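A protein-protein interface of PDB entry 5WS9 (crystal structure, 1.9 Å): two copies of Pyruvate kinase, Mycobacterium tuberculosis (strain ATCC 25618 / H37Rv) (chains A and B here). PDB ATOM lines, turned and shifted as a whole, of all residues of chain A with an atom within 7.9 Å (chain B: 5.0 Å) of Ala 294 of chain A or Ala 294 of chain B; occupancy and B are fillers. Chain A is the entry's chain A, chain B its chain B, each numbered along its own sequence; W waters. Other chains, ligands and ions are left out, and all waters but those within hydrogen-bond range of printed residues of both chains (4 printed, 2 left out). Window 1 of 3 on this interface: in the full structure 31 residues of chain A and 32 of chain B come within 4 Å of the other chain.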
ATOM      1  N   ARG A 245     -22.133   6.134  15.825  1.00  0.00           N
ATOM      2  CA  ARG A 245     -21.953   4.966  14.944  1.00  0.00           C
ATOM      3  C   ARG A 245     -22.816   4.978  13.716  1.00  0.00           C
ATOM      4  O   ARG A 245     -22.476   4.287  12.727  1.00  0.00           O
ATOM      5  CB  ARG A 245     -22.190   3.665  15.740  1.00  0.00           C
ATOM      6  CG  ARG A 245     -21.186   3.539  16.915  1.00  0.00           C
ATOM      7  CD  ARG A 245     -21.347   2.262  17.711  1.00  0.00           C
ATOM      8  NE  ARG A 245     -22.752   1.958  18.025  1.00  0.00           N
ATOM      9  CZ  ARG A 245     -23.138   0.833  18.607  1.00  0.00           C
ATOM     10  NH1 ARG A 245     -24.427   0.575  18.766  1.00  0.00           N
ATOM     11  NH2 ARG A 245     -22.227  -0.070  18.964  1.00  0.00           N
ATOM     12  N   PRO A 258     -16.655  -1.579  14.682  1.00  0.00           N
ATOM     13  CA  PRO A 258     -16.415  -2.200  16.011  1.00  0.00           C
ATOM     14  C   PRO A 258     -15.011  -1.979  16.565  1.00  0.00           C
ATOM     15  O   PRO A 258     -14.863  -1.566  17.731  1.00  0.00           O
ATOM     16  CB  PRO A 258     -16.729  -3.677  15.770  1.00  0.00           C
ATOM     17  CG  PRO A 258     -17.777  -3.633  14.709  1.00  0.00           C
ATOM     18  CD  PRO A 258     -17.320  -2.531  13.762  1.00  0.00           C
ATOM     19  N   GLN A 261     -14.660   1.821  17.523  1.00  0.00           N
ATOM     20  CA  GLN A 261     -15.324   2.053  18.789  1.00  0.00           C
ATOM     21  C   GLN A 261     -14.391   1.728  19.945  1.00  0.00           C
ATOM     22  O   GLN A 261     -14.208   2.532  20.882  1.00  0.00           O
ATOM     23  CB  GLN A 261     -16.613   1.220  18.892  1.00  0.00           C
ATOM     24  CG  GLN A 261     -17.217   1.225  20.287  1.00  0.00           C
ATOM     25  CD  GLN A 261     -18.520   0.463  20.403  1.00  0.00           C
ATOM     26  OE1 GLN A 261     -19.419   0.610  19.551  1.00  0.00           O
ATOM     27  NE2 GLN A 261     -18.664  -0.322  21.490  1.00  0.00           N
ATOM     28  N   ALA A 278     -22.883   5.561  20.949  1.00  0.00           N
ATOM     29  CA  ALA A 278     -24.218   5.974  20.489  1.00  0.00           C
ATOM     30  C   ALA A 278     -24.696   5.224  19.260  1.00  0.00           C
ATOM     31  O   ALA A 278     -23.901   4.804  18.425  1.00  0.00           O
ATOM     32  CB  ALA A 278     -24.236   7.473  20.195  1.00  0.00           C
ATOM     33  N   THR A 279     -26.013   5.029  19.204  1.00  0.00           N
ATOM     34  CA  THR A 279     -26.760   4.789  17.999  1.00  0.00           C
ATOM     35  C   THR A 279     -26.996   3.324  17.715  1.00  0.00           C
ATOM     36  O   THR A 279     -26.062   2.552  17.546  1.00  0.00           O
ATOM     37  CB  THR A 279     -26.167   5.520  16.762  1.00  0.00           C
ATOM     38  OG1 THR A 279     -26.034   6.923  17.072  1.00  0.00           O
ATOM     39  CG2 THR A 279     -27.074   5.376  15.591  1.00  0.00           C
ATOM     40  N   GLN A 280     -28.283   2.984  17.651  1.00  0.00           N
ATOM     41  CA  GLN A 280     -28.815   1.673  17.349  1.00  0.00           C
ATOM     42  C   GLN A 280     -28.484   0.593  18.384  1.00  0.00           C
ATOM     43  O   GLN A 280     -28.609  -0.610  18.107  1.00  0.00           O
ATOM     44  CB  GLN A 280     -28.431   1.227  15.939  1.00  0.00           C
ATOM     45  CG  GLN A 280     -29.118   2.034  14.849  1.00  0.00           C
ATOM     46  CD  GLN A 280     -28.877   1.479  13.468  1.00  0.00           C
ATOM     47  OE1 GLN A 280     -27.794   1.021  13.162  1.00  0.00           O
ATOM     48  NE2 GLN A 280     -29.940   1.428  12.645  1.00  0.00           N
ATOM     49  N   MET A 281     -28.169   1.009  19.598  1.00  0.00           N
ATOM     50  CA  MET A 281     -27.819   0.056  20.624  1.00  0.00           C
ATOM     51  C   MET A 281     -28.972  -0.863  20.950  1.00  0.00           C
ATOM     52  O   MET A 281     -28.757  -2.047  21.162  1.00  0.00           O
ATOM     53  CB  MET A 281     -27.318   0.737  21.884  1.00  0.00           C
ATOM     54  CG  MET A 281     -26.139   1.643  21.641  1.00  0.00           C
ATOM     55  SD  MET A 281     -25.096   1.757  23.108  1.00  0.00           S
ATOM     56  CE  MET A 281     -24.217   0.200  23.013  1.00  0.00           C
ATOM     57  N   LEU A 282     -30.198  -0.336  20.943  1.00  0.00           N
ATOM     58  CA  LEU A 282     -31.390  -1.143  21.186  1.00  0.00           C
ATOM     59  C   LEU A 282     -32.421  -0.837  20.112  1.00  0.00           C
ATOM     60  O   LEU A 282     -33.634  -0.733  20.403  1.00  0.00           O
ATOM     61  CB  LEU A 282     -31.962  -0.803  22.599  1.00  0.00           C
ATOM     62  CG  LEU A 282     -31.138  -1.238  23.824  1.00  0.00           C
ATOM     63  CD1 LEU A 282     -31.747  -0.836  25.165  1.00  0.00           C
ATOM     64  CD2 LEU A 282     -30.875  -2.741  23.838  1.00  0.00           C
ATOM     65  N   ASP A 283     -31.929  -0.652  18.883  1.00  0.00           N
ATOM     66  CA  ASP A 283     -32.735  -0.110  17.765  1.00  0.00           C
ATOM     67  C   ASP A 283     -34.135  -0.757  17.644  1.00  0.00           C
ATOM     68  O   ASP A 283     -35.113  -0.063  17.396  1.00  0.00           O
ATOM     69  CB  ASP A 283     -31.968  -0.297  16.418  1.00  0.00           C
ATOM     70  CG  ASP A 283     -32.649   0.398  15.255  1.00  0.00           C
ATOM     71  OD1 ASP A 283     -32.618   1.601  15.242  1.00  0.00           O
ATOM     72  OD2 ASP A 283     -33.261  -0.263  14.375  1.00  0.00           O
ATOM     73  N   SER A 284     -34.211  -2.074  17.722  1.00  0.00           N
ATOM     74  CA  SER A 284     -35.490  -2.776  17.482  1.00  0.00           C
ATOM     75  C   SER A 284     -36.554  -2.392  18.529  1.00  0.00           C
ATOM     76  O   SER A 284     -37.753  -2.639  18.336  1.00  0.00           O
ATOM     77  CB  SER A 284     -35.287  -4.290  17.473  1.00  0.00           C
ATOM     78  OG  SER A 284     -34.978  -4.771  18.773  1.00  0.00           O
ATOM     79  N   PRO A 291     -35.521  -6.251  23.120  1.00  0.00           N
ATOM     80  CA  PRO A 291     -34.519  -6.071  22.074  1.00  0.00           C
ATOM     81  C   PRO A 291     -34.111  -7.425  21.410  1.00  0.00           C
ATOM     82  O   PRO A 291     -34.485  -8.512  21.893  1.00  0.00           O
ATOM     83  CB  PRO A 291     -33.343  -5.477  22.842  1.00  0.00           C
ATOM     84  CG  PRO A 291     -33.421  -6.147  24.180  1.00  0.00           C
ATOM     85  CD  PRO A 291     -34.904  -6.265  24.465  1.00  0.00           C
ATOM     86  N   THR A 292     -33.330  -7.352  20.349  1.00  0.00           N
ATOM     87  CA  THR A 292     -32.730  -8.548  19.776  1.00  0.00           C
ATOM     88  C   THR A 292     -31.506  -9.003  20.613  1.00  0.00           C
ATOM     89  O   THR A 292     -31.014  -8.291  21.475  1.00  0.00           O
ATOM     90  CB  THR A 292     -32.245  -8.314  18.326  1.00  0.00           C
ATOM     91  OG1 THR A 292     -31.082  -7.463  18.347  1.00  0.00           O
ATOM     92  CG2 THR A 292     -33.356  -7.709  17.447  1.00  0.00           C
ATOM     93  N   ARG A 293     -31.045 -10.203  20.348  1.00  0.00           N
ATOM     94  CA  ARG A 293     -29.896 -10.733  21.064  1.00  0.00           C
ATOM     95  C   ARG A 293     -28.609  -9.957  20.665  1.00  0.00           C
ATOM     96  O   ARG A 293     -27.659  -9.816  21.456  1.00  0.00           O
ATOM     97  CB  ARG A 293     -29.764 -12.222  20.737  1.00  0.00           C
ATOM     98  CG  ARG A 293     -31.028 -13.019  21.073  1.00  0.00           C
ATOM     99  CD  ARG A 293     -31.318 -13.020  22.562  1.00  0.00           C
ATOM    100  NE  ARG A 293     -32.583 -13.695  22.814  1.00  0.00           N
ATOM    101  CZ  ARG A 293     -33.766 -13.110  22.884  1.00  0.00           C
ATOM    102  NH1 ARG A 293     -33.865 -11.791  22.824  1.00  0.00           N
ATOM    103  NH2 ARG A 293     -34.874 -13.848  23.024  1.00  0.00           N
ATOM    104  N   ALA A 294     -28.559  -9.465  19.446  1.00  0.00           N
ATOM    105  CA  ALA A 294     -27.428  -8.644  19.022  1.00  0.00           C
ATOM    106  C   ALA A 294     -27.395  -7.364  19.807  1.00  0.00           C
ATOM    107  O   ALA A 294     -26.323  -6.833  20.128  1.00  0.00           O
ATOM    108  CB  ALA A 294     -27.483  -8.342  17.514  1.00  0.00           C
ATOM    109  N   GLU A 295     -28.572  -6.834  20.089  1.00  0.00           N
ATOM    110  CA  GLU A 295     -28.671  -5.574  20.782  1.00  0.00           C
ATOM    111  C   GLU A 295     -28.222  -5.685  22.248  1.00  0.00           C
ATOM    112  O   GLU A 295     -27.484  -4.840  22.737  1.00  0.00           O
ATOM    113  CB  GLU A 295     -30.067  -5.008  20.613  1.00  0.00           C
ATOM    114  CG  GLU A 295     -30.247  -4.362  19.257  1.00  0.00           C
ATOM    115  CD  GLU A 295     -31.728  -4.235  18.803  1.00  0.00           C
ATOM    116  OE1 GLU A 295     -32.656  -4.662  19.544  1.00  0.00           O
ATOM    117  OE2 GLU A 295     -31.952  -3.832  17.614  1.00  0.00           O
ATOM    118  N   ALA A 296     -28.654  -6.724  22.934  1.00  0.00           N
ATOM    119  CA  ALA A 296     -28.199  -6.953  24.283  1.00  0.00           C
ATOM    120  C   ALA A 296     -26.675  -7.159  24.301  1.00  0.00           C
ATOM    121  O   ALA A 296     -25.987  -6.716  25.211  1.00  0.00           O
ATOM    122  CB  ALA A 296     -28.888  -8.157  24.880  1.00  0.00           C
ATOM    123  N   SER A 297     -26.160  -7.859  23.315  1.00  0.00           N
ATOM    124  CA  SER A 297     -24.745  -8.094  23.213  1.00  0.00           C
ATOM    125  C   SER A 297     -23.967  -6.762  23.030  1.00  0.00           C
ATOM    126  O   SER A 297     -22.889  -6.532  23.633  1.00  0.00           O
ATOM    127  CB  SER A 297     -24.485  -9.027  22.048  1.00  0.00           C
ATOM    128  OG  SER A 297     -23.133  -9.063  21.710  1.00  0.00           O
ATOM    129  N   ASP A 298     -24.469  -5.923  22.145  1.00  0.00           N
ATOM    130  CA  ASP A 298     -23.861  -4.653  21.851  1.00  0.00           C
ATOM    131  C   ASP A 298     -23.771  -3.781  23.106  1.00  0.00           C
ATOM    132  O   ASP A 298     -22.700  -3.250  23.410  1.00  0.00           O
ATOM    133  CB  ASP A 298     -24.645  -3.961  20.755  1.00  0.00           C
ATOM    134  CG  ASP A 298     -24.062  -2.651  20.351  1.00  0.00           C
ATOM    135  OD1 ASP A 298     -22.859  -2.577  20.111  1.00  0.00           O
ATOM    136  OD2 ASP A 298     -24.843  -1.680  20.245  1.00  0.00           O
ATOM    137  N   VAL A 299     -24.856  -3.730  23.880  1.00  0.00           N
ATOM    138  CA  VAL A 299     -24.860  -2.979  25.141  1.00  0.00           C
ATOM    139  C   VAL A 299     -23.842  -3.554  26.136  1.00  0.00           C
ATOM    140  O   VAL A 299     -23.008  -2.838  26.656  1.00  0.00           O
ATOM    141  CB  VAL A 299     -26.258  -2.925  25.752  1.00  0.00           C
ATOM    142  CG1 VAL A 299     -26.231  -2.361  27.148  1.00  0.00           C
ATOM    143  CG2 VAL A 299     -27.195  -2.149  24.856  1.00  0.00           C
ATOM    144  N   ALA A 300     -23.888  -4.856  26.354  1.00  0.00           N
ATOM    145  CA  ALA A 300     -22.945  -5.514  27.269  1.00  0.00           C
ATOM    146  C   ALA A 300     -21.505  -5.281  26.863  1.00  0.00           C
ATOM    147  O   ALA A 300     -20.651  -5.023  27.723  1.00  0.00           O
ATOM    148  CB  ALA A 300     -23.217  -7.009  27.347  1.00  0.00           C
ATOM    149  N   ASN A 301     -21.216  -5.377  25.566  1.00  0.00           N
ATOM    150  CA  ASN A 301     -19.825  -5.271  25.120  1.00  0.00           C
ATOM    151  C   ASN A 301     -19.310  -3.837  25.193  1.00  0.00           C
ATOM    152  O   ASN A 301     -18.114  -3.623  25.440  1.00  0.00           O
ATOM    153  CB  ASN A 301     -19.651  -5.849  23.709  1.00  0.00           C
ATOM    154  CG  ASN A 301     -19.494  -7.335  23.721  1.00  0.00           C
ATOM    155  OD1 ASN A 301     -18.486  -7.832  24.234  1.00  0.00           O
ATOM    156  ND2 ASN A 301     -20.459  -8.070  23.101  1.00  0.00           N
ATOM    157  N   GLU A 315     -34.919   5.161  20.098  1.00  0.00           N
ATOM    158  CA  GLU A 315     -35.522   4.301  21.123  1.00  0.00           C
ATOM    159  C   GLU A 315     -36.280   5.088  22.170  1.00  0.00           C
ATOM    160  O   GLU A 315     -37.308   4.601  22.699  1.00  0.00           O
ATOM    161  CB  GLU A 315     -34.441   3.437  21.802  1.00  0.00           C
ATOM    162  CG  GLU A 315     -33.678   2.563  20.840  1.00  0.00           C
ATOM    163  CD  GLU A 315     -32.296   3.134  20.483  1.00  0.00           C
ATOM    164  OE1 GLU A 315     -32.205   4.336  20.221  1.00  0.00           O
ATOM    165  OE2 GLU A 315     -31.304   2.367  20.487  1.00  0.00           O
ATOM    166  N   ARG B 245     -29.142 -18.387  21.169  1.00  0.00           N
ATOM    167  CA  ARG B 245     -29.468 -17.201  21.972  1.00  0.00           C
ATOM    168  C   ARG B 245     -30.936 -16.822  21.948  1.00  0.00           C
ATOM    169  O   ARG B 245     -31.404 -16.114  22.869  1.00  0.00           O
ATOM    170  CB  ARG B 245     -28.601 -15.999  21.512  1.00  0.00           C
ATOM    171  CG  ARG B 245     -27.095 -16.302  21.651  1.00  0.00           C
ATOM    172  CD  ARG B 245     -26.198 -15.155  21.264  1.00  0.00           C
ATOM    173  NE  ARG B 245     -26.598 -14.523  20.009  1.00  0.00           N
ATOM    174  CZ  ARG B 245     -26.037 -13.429  19.525  1.00  0.00           C
ATOM    175  NH1 ARG B 245     -26.535 -12.861  18.433  1.00  0.00           N
ATOM    176  NH2 ARG B 245     -25.024 -12.851  20.192  1.00  0.00           N
ATOM    177  N   GLN B 280     -30.034 -14.086  15.530  1.00  0.00           N
ATOM    178  CA  GLN B 280     -30.194 -12.638  15.442  1.00  0.00           C
ATOM    179  C   GLN B 280     -28.914 -11.838  15.292  1.00  0.00           C
ATOM    180  O   GLN B 280     -28.921 -10.612  15.481  1.00  0.00           O
ATOM    181  CB  GLN B 280     -31.041 -12.099  16.602  1.00  0.00           C
ATOM    182  CG  GLN B 280     -32.483 -12.549  16.563  1.00  0.00           C
ATOM    183  CD  GLN B 280     -33.324 -11.888  17.617  1.00  0.00           C
ATOM    184  OE1 GLN B 280     -32.864 -11.617  18.712  1.00  0.00           O
ATOM    185  NE2 GLN B 280     -34.568 -11.540  17.251  1.00  0.00           N
ATOM    186  N   MET B 281     -27.847 -12.485  14.838  1.00  0.00           N
ATOM    187  CA  MET B 281     -26.583 -11.791  14.687  1.00  0.00           C
ATOM    188  C   MET B 281     -26.677 -10.663  13.687  1.00  0.00           C
ATOM    189  O   MET B 281     -26.094  -9.617  13.904  1.00  0.00           O
ATOM    190  CB  MET B 281     -25.462 -12.743  14.308  1.00  0.00           C
ATOM    191  CG  MET B 281     -25.283 -13.880  15.290  1.00  0.00           C
ATOM    192  SD  MET B 281     -23.574 -14.467  15.312  1.00  0.00           S
ATOM    193  CE  MET B 281     -22.841 -13.167  16.302  1.00  0.00           C
ATOM    194  N   THR B 292     -27.759  -3.259  11.326  1.00  0.00           N
ATOM    195  CA  THR B 292     -27.600  -2.188  12.308  1.00  0.00           C
ATOM    196  C   THR B 292     -26.170  -2.194  12.906  1.00  0.00           C
ATOM    197  O   THR B 292     -25.412  -3.115  12.735  1.00  0.00           O
ATOM    198  CB  THR B 292     -28.607  -2.316  13.466  1.00  0.00           C
ATOM    199  OG1 THR B 292     -28.210  -3.417  14.296  1.00  0.00           O
ATOM    200  CG2 THR B 292     -30.055  -2.493  12.943  1.00  0.00           C
ATOM    201  N   ARG B 293     -25.824  -1.123  13.580  1.00  0.00           N
ATOM    202  CA  ARG B 293     -24.532  -1.004  14.194  1.00  0.00           C
ATOM    203  C   ARG B 293     -24.415  -2.006  15.388  1.00  0.00           C
ATOM    204  O   ARG B 293     -23.321  -2.494  15.708  1.00  0.00           O
ATOM    205  CB  ARG B 293     -24.356   0.444  14.684  1.00  0.00           C
ATOM    206  CG  ARG B 293     -24.526   1.471  13.566  1.00  0.00           C
ATOM    207  CD  ARG B 293     -23.453   1.350  12.494  1.00  0.00           C
ATOM    208  NE  ARG B 293     -23.750   2.293  11.429  1.00  0.00           N
ATOM    209  CZ  ARG B 293     -24.408   2.004  10.317  1.00  0.00           C
ATOM    210  NH1 ARG B 293     -24.783   0.757  10.072  1.00  0.00           N
ATOM    211  NH2 ARG B 293     -24.717   2.969   9.452  1.00  0.00           N
ATOM    212  N   ALA B 294     -25.524  -2.322  16.041  1.00  0.00           N
ATOM    213  CA  ALA B 294     -25.493  -3.325  17.100  1.00  0.00           C
ATOM    214  C   ALA B 294     -25.154  -4.680  16.522  1.00  0.00           C
ATOM    215  O   ALA B 294     -24.444  -5.477  17.128  1.00  0.00           O
ATOM    216  CB  ALA B 294     -26.808  -3.390  17.863  1.00  0.00           C
ATOM    217  N   GLU B 295     -25.688  -4.941  15.347  1.00  0.00           N
ATOM    218  CA  GLU B 295     -25.465  -6.210  14.688  1.00  0.00           C
ATOM    219  C   GLU B 295     -24.010  -6.403  14.245  1.00  0.00           C
ATOM    220  O   GLU B 295     -23.428  -7.473  14.450  1.00  0.00           O
ATOM    221  CB  GLU B 295     -26.460  -6.367  13.553  1.00  0.00           C
ATOM    222  CG  GLU B 295     -27.836  -6.751  14.067  1.00  0.00           C
ATOM    223  CD  GLU B 295     -28.993  -6.422  13.111  1.00  0.00           C
ATOM    224  OE1 GLU B 295     -28.736  -5.894  11.986  1.00  0.00           O
ATOM    225  OE2 GLU B 295     -30.199  -6.590  13.539  1.00  0.00           O
ATOM    226  N   ALA B 296     -23.425  -5.393  13.638  1.00  0.00           N
ATOM    227  CA  ALA B 296     -22.018  -5.475  13.281  1.00  0.00           C
ATOM    228  C   ALA B 296     -21.158  -5.666  14.544  1.00  0.00           C
ATOM    229  O   ALA B 296     -20.159  -6.377  14.532  1.00  0.00           O
ATOM    230  CB  ALA B 296     -21.583  -4.226  12.552  1.00  0.00           C
ATOM    231  N   SER B 297     -21.523  -4.978  15.613  1.00  0.00           N
ATOM    232  CA  SER B 297     -20.800  -5.103  16.860  1.00  0.00           C
ATOM    233  C   SER B 297     -20.883  -6.559  17.427  1.00  0.00           C
ATOM    234  O   SER B 297     -19.897  -7.133  17.948  1.00  0.00           O
ATOM    235  CB  SER B 297     -21.388  -4.122  17.861  1.00  0.00           C
ATOM    236  OG  SER B 297     -20.933  -4.360  19.174  1.00  0.00           O
ATOM    237  N   ASP B 298     -22.075  -7.108  17.396  1.00  0.00           N
ATOM    238  CA  ASP B 298     -22.339  -8.448  17.883  1.00  0.00           C
ATOM    239  C   ASP B 298     -21.495  -9.485  17.129  1.00  0.00           C
ATOM    240  O   ASP B 298     -20.837 -10.312  17.744  1.00  0.00           O
ATOM    241  CB  ASP B 298     -23.816  -8.745  17.755  1.00  0.00           C
ATOM    242  CG  ASP B 298     -24.196 -10.094  18.273  1.00  0.00           C
ATOM    243  OD1 ASP B 298     -23.789 -10.463  19.380  1.00  0.00           O
ATOM    244  OD2 ASP B 298     -24.946 -10.795  17.566  1.00  0.00           O
HETATM  245  O   HOH W   1     -30.296  -8.059  15.830  1.00  0.00           O
HETATM  246  O   HOH W   2     -29.752  -2.626  16.430  1.00  0.00           O
HETATM  247  O   HOH W   3     -20.626  -2.392  21.646  1.00  0.00           O
HETATM  248  O   HOH W   4     -21.350 -11.426  20.216  1.00  0.00           O
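The guanidinium group (NE) of Arg 293 of chain B sits at hydrogen-bond distance from the backbone carbonyl oxygen (O) of Arg 245 of chain A (2.7 Å).
OE1 of Gln 280 of chain A is in hydrogen-bond range of N of Arg 293 of chain B, 2.9 Å away.
NE of Arg 293 of chain A lies within hydrogen-bond range of O of Arg 245 of chain B (2.7 Å).
N of Arg 293 of chain A is in hydrogen-bond range of OE1 of Gln 280 of chain B.
The side-chain hydroxyl (OG) of Ser 297 of chain A is in hydrogen-bond range of the side-chain carboxylate (OD1) of Asp 298 of chain B.
OD1 of Asp 298 of chain A lies within hydrogen-bond range of OG of Ser 297 of chain B (2.8 Å).
NE of Arg 245 of chain A lies within hydrogen-bond range of O of Ala 278 of chain A.
N of Asp 283 of chain A sits at hydrogen-bond distance from OE2 of Glu 295 of chain A.
The side-chain hydroxyl (OG) of Ser 284 of chain A is in hydrogen-bond range of the backbone NH (N) of Thr 292 of chain A, at 3.4 Å.
N of Ala 294 of chain A lies close to OG1 of Thr 292 of chain A, 3.4 Å away.
The side-chain hydroxyl (OG1) of Thr 292 of chain B sits close to the backbone NH (N) of Ala 294 of chain B (3.4 Å).
N of Thr 292 of chain B lies within hydrogen-bond range of OE1 of Glu 295 of chain B (2.9 Å).
Pro 258 of chain A touches Ala 296 of chain B.
Pro 258 of chain A touches Ser 297 of chain B (CG to CA, 3.99 Å).
Arg 293 of chain B touches Thr 279 of chain A.
Ala 294 of chain B touches Gln 280 of chain A.
CB of Ala 294 of chain A touches O of Gln 280 of chain B (3.4 Å).
O of Ala 294 of chain B touches O of Ala 294 of chain A (3.8 Å).
Ala 294 of chain A touches Glu 295 of chain B.
Ala 294 of chain A touches Asp 298 of chain B (CB to OD2, 3.5 Å).
Ala 294 of chain B touches Glu 295 of chain A.
CB of Ala 294 of chain B touches OD2 of Asp 298 of chain A, at 3.5 Å.
Of the printed residues of chain B, Pro 258 of chain A touches Ala 296 (3.6 Å) and Ser 297 (3.99 Å).
Of the printed residues of chain B, Gln 280 of chain A touches Thr 292 (3.3 Å), Arg 293 (2.9 Å) and Ala 294 (3.3 Å).
Of the printed residues of chain B, Thr 292 of chain A touches Gln 280 (3.3 Å).
Printed residues of chain B within 4 Å of Ala 294 of chain A: Gln 280, Ala 294, Glu 295 and Asp 298.
Val 299 of chain A touches none of the printed residues of chain B.
Printed residues of chain A within 4 Å of Thr 292 of chain B: Gln 280 (3.3 Å).
Ala 294 of chain B touches four residues of chain A.
Of the printed residues of chain A, Asp 298 of chain B touches Ala 294 (3.5 Å) and Ser 297 (2.8 Å).
The nearest printed residue of chain B that does not touch Ala 294 of chain A is Met 281 of chain B (4.1 Å).
The nearest printed residue of chain B that does not touch Arg 293 of chain A is Asp 298 of chain B (4.4 Å).
Of the 22 printed residues of chain A, 10 touch a printed residue of chain B.
Hydrophobic or aromatic side chains of chain A within 4 Å of the printed part of chain B: Pro 258 and Ala 294.
Among the printed residues, no Asp or Glu carboxylate lies within 4 Å of a Lys or Arg side-chain nitrogen of the other chain.
Arg 245 of chain A touches Arg 293 of chain B, and with the chains exchanged Arg 293 of chain A touches Arg 245 of chain B.
Ala 294 of chain B touches its own counterpart, Ala 294 of chain A.
Ala 294 of chain A touches Glu 295 of chain B, and with the chains exchanged Glu 295 of chain A touches Ala 294 of chain B.
Ala 294 of chain A touches Asp 298 of chain B, and with the chains exchanged Asp 298 of chain A touches Ala 294 of chain B.
Of the 18 pairs that touch across the chains among the printed residues, 15 have their exchanged pair printed and touching as well.
Water W1 lies within hydrogen-bond range of OG1 of Thr 292 of chain A (2.7 Å), OE2 of Glu 295 of chain B (2.7 Å) and O of Gln 280 of chain B (2.9 Å).
Water W3 lies within hydrogen-bond range of OD1 of Asp 298 of chain A (2.7 Å), NE2 of Gln 261 of chain A (2.9 Å) and OG of Ser 297 of chain B (3.2 Å).
Water W2 lies within hydrogen-bond range of the side-chain hydroxyl (OG1) of Thr 292 of chain B (2.7 Å), the side-chain carboxylate (OE2) of Glu 295 of chain A (2.8 Å) and the backbone carbonyl oxygen (O) of Gln 280 of chain A (2.9 Å).
Water W4 bridges OD1 of Asp 298 of chain B (2.8 Å) and OG of Ser 297 of chain A (3.3 Å).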
